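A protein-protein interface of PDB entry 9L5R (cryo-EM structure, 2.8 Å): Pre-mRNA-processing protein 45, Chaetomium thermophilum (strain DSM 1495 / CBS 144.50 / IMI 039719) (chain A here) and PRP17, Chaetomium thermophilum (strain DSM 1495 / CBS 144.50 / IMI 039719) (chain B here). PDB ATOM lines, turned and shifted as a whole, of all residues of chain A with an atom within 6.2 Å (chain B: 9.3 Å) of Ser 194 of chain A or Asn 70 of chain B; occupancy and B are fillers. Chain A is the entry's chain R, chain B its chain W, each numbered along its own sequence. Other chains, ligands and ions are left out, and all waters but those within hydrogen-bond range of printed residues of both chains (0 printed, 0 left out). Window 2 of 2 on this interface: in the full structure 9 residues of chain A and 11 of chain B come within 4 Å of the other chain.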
ATOM      1  N   TYR A 191     -22.711   7.962  16.657  1.00  0.00           N
ATOM      2  CA  TYR A 191     -22.528   6.921  17.677  1.00  0.00           C
ATOM      3  C   TYR A 191     -21.552   5.775  17.417  1.00  0.00           C
ATOM      4  O   TYR A 191     -21.974   4.673  17.057  1.00  0.00           O
ATOM      5  CB  TYR A 191     -23.849   6.298  18.101  1.00  0.00           C
ATOM      6  CG  TYR A 191     -23.683   5.615  19.445  1.00  0.00           C
ATOM      7  CD1 TYR A 191     -22.942   6.213  20.461  1.00  0.00           C
ATOM      8  CD2 TYR A 191     -24.226   4.368  19.686  1.00  0.00           C
ATOM      9  CE1 TYR A 191     -22.771   5.593  21.676  1.00  0.00           C
ATOM     10  CE2 TYR A 191     -24.060   3.748  20.894  1.00  0.00           C
ATOM     11  CZ  TYR A 191     -23.332   4.360  21.880  1.00  0.00           C
ATOM     12  OH  TYR A 191     -23.181   3.723  23.081  1.00  0.00           O
ATOM     13  N   THR A 192     -20.257   6.020  17.536  1.00  0.00           N
ATOM     14  CA  THR A 192     -19.315   4.912  17.688  1.00  0.00           C
ATOM     15  C   THR A 192     -19.384   4.352  19.106  1.00  0.00           C
ATOM     16  O   THR A 192     -19.069   5.073  20.060  1.00  0.00           O
ATOM     17  CB  THR A 192     -17.899   5.371  17.390  1.00  0.00           C
ATOM     18  OG1 THR A 192     -17.885   6.109  16.163  1.00  0.00           O
ATOM     19  CG2 THR A 192     -16.979   4.181  17.268  1.00  0.00           C
ATOM     20  N   PRO A 193     -19.766   3.090  19.292  1.00  0.00           N
ATOM     21  CA  PRO A 193     -19.831   2.522  20.641  1.00  0.00           C
ATOM     22  C   PRO A 193     -18.467   2.101  21.167  1.00  0.00           C
ATOM     23  O   PRO A 193     -17.524   1.851  20.418  1.00  0.00           O
ATOM     24  CB  PRO A 193     -20.733   1.293  20.466  1.00  0.00           C
ATOM     25  CG  PRO A 193     -21.304   1.393  19.103  1.00  0.00           C
ATOM     26  CD  PRO A 193     -20.326   2.166  18.299  1.00  0.00           C
ATOM     27  N   SER A 194     -18.386   2.019  22.494  1.00  0.00           N
ATOM     28  CA  SER A 194     -17.316   1.305  23.180  1.00  0.00           C
ATOM     29  C   SER A 194     -17.713  -0.169  23.255  1.00  0.00           C
ATOM     30  O   SER A 194     -18.631  -0.599  22.552  1.00  0.00           O
ATOM     31  CB  SER A 194     -17.037   1.931  24.546  1.00  0.00           C
ATOM     32  OG  SER A 194     -16.462   3.216  24.410  1.00  0.00           O
ATOM     33  N   ALA A 195     -17.029  -0.966  24.076  1.00  0.00           N
ATOM     34  CA  ALA A 195     -17.095  -2.408  23.872  1.00  0.00           C
ATOM     35  C   ALA A 195     -18.436  -3.044  24.235  1.00  0.00           C
ATOM     36  O   ALA A 195     -19.235  -3.320  23.333  1.00  0.00           O
ATOM     37  CB  ALA A 195     -15.980  -3.077  24.677  1.00  0.00           C
ATOM     38  N   GLN A 196     -18.722  -3.191  25.534  1.00  0.00           N
ATOM     39  CA  GLN A 196     -19.945  -3.807  26.057  1.00  0.00           C
ATOM     40  C   GLN A 196     -19.814  -3.741  27.575  1.00  0.00           C
ATOM     41  O   GLN A 196     -18.834  -3.179  28.073  1.00  0.00           O
ATOM     42  CB  GLN A 196     -20.122  -5.253  25.547  1.00  0.00           C
ATOM     43  CG  GLN A 196     -21.465  -5.963  25.786  1.00  0.00           C
ATOM     44  CD  GLN A 196     -22.644  -5.229  25.169  1.00  0.00           C
ATOM     45  OE1 GLN A 196     -22.743  -5.115  23.948  1.00  0.00           O
ATOM     46  NE2 GLN A 196     -23.550  -4.735  26.014  1.00  0.00           N
ATOM     47  N   THR A 201     -15.549  -7.668  22.086  1.00  0.00           N
ATOM     48  CA  THR A 201     -15.686  -7.702  20.638  1.00  0.00           C
ATOM     49  C   THR A 201     -16.279  -6.396  20.119  1.00  0.00           C
ATOM     50  O   THR A 201     -17.161  -5.796  20.740  1.00  0.00           O
ATOM     51  CB  THR A 201     -16.533  -8.910  20.212  1.00  0.00           C
ATOM     52  OG1 THR A 201     -16.567  -9.001  18.782  1.00  0.00           O
ATOM     53  CG2 THR A 201     -17.953  -8.864  20.779  1.00  0.00           C
ATOM     54  N   LYS A 203     -18.429  -3.943  17.737  1.00  0.00           N
ATOM     55  CA  LYS A 203     -19.734  -4.065  17.112  1.00  0.00           C
ATOM     56  C   LYS A 203     -20.115  -2.753  16.445  1.00  0.00           C
ATOM     57  O   LYS A 203     -19.427  -1.737  16.568  1.00  0.00           O
ATOM     58  CB  LYS A 203     -20.787  -4.538  18.116  1.00  0.00           C
ATOM     59  CG  LYS A 203     -20.814  -3.797  19.425  1.00  0.00           C
ATOM     60  CD  LYS A 203     -21.861  -4.425  20.315  1.00  0.00           C
ATOM     61  CE  LYS A 203     -21.515  -5.877  20.605  1.00  0.00           C
ATOM     62  NZ  LYS A 203     -22.507  -6.542  21.492  1.00  0.00           N
ATOM     63  N   LYS B  69     -10.886   8.995  22.778  1.00  0.00           N
ATOM     64  CA  LYS B  69     -11.263   9.758  23.960  1.00  0.00           C
ATOM     65  C   LYS B  69     -12.777   9.956  24.000  1.00  0.00           C
ATOM     66  O   LYS B  69     -13.308  10.923  23.453  1.00  0.00           O
ATOM     67  CB  LYS B  69     -10.530  11.099  23.983  1.00  0.00           C
ATOM     68  CG  LYS B  69      -9.007  10.963  24.039  1.00  0.00           C
ATOM     69  CD  LYS B  69      -8.331  12.294  24.314  1.00  0.00           C
ATOM     70  CE  LYS B  69      -8.354  13.197  23.094  1.00  0.00           C
ATOM     71  NZ  LYS B  69      -7.631  14.474  23.331  1.00  0.00           N
ATOM     72  N   ASN B  70     -13.457   9.022  24.663  1.00  0.00           N
ATOM     73  CA  ASN B  70     -14.912   8.971  24.650  1.00  0.00           C
ATOM     74  C   ASN B  70     -15.516  10.120  25.445  1.00  0.00           C
ATOM     75  O   ASN B  70     -15.065  10.435  26.549  1.00  0.00           O
ATOM     76  CB  ASN B  70     -15.392   7.641  25.224  1.00  0.00           C
ATOM     77  CG  ASN B  70     -15.194   6.488  24.271  1.00  0.00           C
ATOM     78  OD1 ASN B  70     -15.501   5.345  24.596  1.00  0.00           O
ATOM     79  ND2 ASN B  70     -14.695   6.783  23.081  1.00  0.00           N
ATOM     80  N   ASN B  71     -16.544  10.743  24.879  1.00  0.00           N
ATOM     81  CA  ASN B  71     -17.304  11.766  25.578  1.00  0.00           C
ATOM     82  C   ASN B  71     -18.602  11.239  26.178  1.00  0.00           C
ATOM     83  O   ASN B  71     -19.138  11.855  27.108  1.00  0.00           O
ATOM     84  CB  ASN B  71     -17.563  12.950  24.636  1.00  0.00           C
ATOM     85  CG  ASN B  71     -18.334  12.565  23.377  1.00  0.00           C
ATOM     86  OD1 ASN B  71     -18.780  11.433  23.208  1.00  0.00           O
ATOM     87  ND2 ASN B  71     -18.493  13.528  22.485  1.00  0.00           N
ATOM     88  N   VAL B  72     -19.105  10.126  25.675  1.00  0.00           N
ATOM     89  CA  VAL B  72     -20.227   9.409  26.262  1.00  0.00           C
ATOM     90  C   VAL B  72     -19.645   8.275  27.094  1.00  0.00           C
ATOM     91  O   VAL B  72     -18.559   7.769  26.807  1.00  0.00           O
ATOM     92  CB  VAL B  72     -21.188   8.925  25.145  1.00  0.00           C
ATOM     93  CG1 VAL B  72     -22.287   7.993  25.647  1.00  0.00           C
ATOM     94  CG2 VAL B  72     -21.819  10.117  24.484  1.00  0.00           C
ATOM     95  N   LEU B  73     -20.340   7.911  28.171  1.00  0.00           N
ATOM     96  CA  LEU B  73     -19.863   6.871  29.073  1.00  0.00           C
ATOM     97  C   LEU B  73     -19.826   5.494  28.421  1.00  0.00           C
ATOM     98  O   LEU B  73     -19.159   4.597  28.944  1.00  0.00           O
ATOM     99  CB  LEU B  73     -20.752   6.836  30.311  1.00  0.00           C
ATOM    100  CG  LEU B  73     -20.189   6.371  31.642  1.00  0.00           C
ATOM    101  CD1 LEU B  73     -19.051   7.276  32.044  1.00  0.00           C
ATOM    102  CD2 LEU B  73     -21.296   6.405  32.676  1.00  0.00           C
ATOM    103  N   THR B  74     -20.516   5.306  27.297  1.00  0.00           N
ATOM    104  CA  THR B  74     -20.595   4.015  26.625  1.00  0.00           C
ATOM    105  C   THR B  74     -20.022   4.038  25.217  1.00  0.00           C
ATOM    106  O   THR B  74     -20.222   3.078  24.468  1.00  0.00           O
ATOM    107  CB  THR B  74     -22.047   3.538  26.565  1.00  0.00           C
ATOM    108  OG1 THR B  74     -22.860   4.569  25.995  1.00  0.00           O
ATOM    109  CG2 THR B  74     -22.556   3.223  27.937  1.00  0.00           C
ATOM    110  N   GLY B  75     -19.337   5.096  24.826  1.00  0.00           N
ATOM    111  CA  GLY B  75     -18.845   5.196  23.475  1.00  0.00           C
ATOM    112  C   GLY B  75     -18.591   6.637  23.100  1.00  0.00           C
ATOM    113  O   GLY B  75     -18.513   7.508  23.952  1.00  0.00           O
ATOM    114  N   HIS B  76     -18.451   6.862  21.800  1.00  0.00           N
ATOM    115  CA  HIS B  76     -18.229   8.191  21.255  1.00  0.00           C
ATOM    116  C   HIS B  76     -19.425   8.581  20.402  1.00  0.00           C
ATOM    117  O   HIS B  76     -19.796   7.850  19.481  1.00  0.00           O
ATOM    118  CB  HIS B  76     -16.947   8.239  20.425  1.00  0.00           C
ATOM    119  CG  HIS B  76     -16.562   9.618  19.998  1.00  0.00           C
ATOM    120  ND1 HIS B  76     -16.258  10.615  20.898  1.00  0.00           N
ATOM    121  CD2 HIS B  76     -16.437  10.169  18.770  1.00  0.00           C
ATOM    122  CE1 HIS B  76     -15.962  11.721  20.243  1.00  0.00           C
ATOM    123  NE2 HIS B  76     -16.065  11.478  18.950  1.00  0.00           N
ATOM    124  N   ALA B  77     -20.026   9.725  20.715  1.00  0.00           N
ATOM    125  CA  ALA B  77     -21.159  10.254  19.972  1.00  0.00           C
ATOM    126  C   ALA B  77     -20.770  11.573  19.326  1.00  0.00           C
ATOM    127  O   ALA B  77     -20.212  12.451  19.988  1.00  0.00           O
ATOM    128  CB  ALA B  77     -22.369  10.456  20.876  1.00  0.00           C
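The side-chain hydroxyl of Ser 194 of chain A sits close to the side-chain amide oxygen of Asn 70 of chain B, at 2.3 Å.
N of Gly 75 of chain B lies close to OG of Ser 194 of chain A (3.5 Å).
O of Thr 192 of chain A lies within hydrogen-bond range of N of His 76 of chain B.
O of Thr 74 of chain B is in hydrogen-bond range of N of Ser 194 of chain A (2.9 Å).
The side-chain hydroxyl of Tyr 191 of chain A lies within hydrogen-bond range of the side-chain hydroxyl of Thr 74 of chain B, at 3.1 Å.
Among the printed residues, merely in contact across the chains: Tyr 191 of chain A with His 76 of chain B (3.4 Å), Thr 192 of chain A with Gly 75 of chain B (3.4 Å), Pro 193 of chain A with Thr 74 of chain B (3.9 Å) and Pro 193 of chain A with Gly 75 of chain B (3.9 Å).
Printed residues of chain B within 4 Å of Thr 192 of chain A: Gly 75 (3.4 Å) and His 76 (2.6 Å).
Pro 193 of chain A touches just these residues of chain B: Thr 74 (3.9 Å) and Gly 75 (3.9 Å).
Ser 194 of chain A touches three residues of chain B.
Printed residues of chain A within 4 Å of Asn 70 of chain B: Ser 194 (2.3 Å).
Asn 71 of chain B touches none of the printed residues of chain A.
Of the printed residues of chain A, His 76 of chain B touches Tyr 191 and Thr 192.
The nearest residue of chain B that does not touch Ser 194 of chain A is His 76 of chain B (4.9 Å).
Printed residues of chain B that touch a printed residue of chain A: Asn 70, Thr 74, Gly 75 and His 76.
Hydrophobic or aromatic side chains of chain B that line the printed part of chain A: His 76.
Of the 8 printed residues of chain A, 4 touch a printed residue of chain B.
Among the printed residues, no Asp or Glu carboxylate lies within 4 Å of a Lys or Arg side-chain nitrogen of the other chain.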
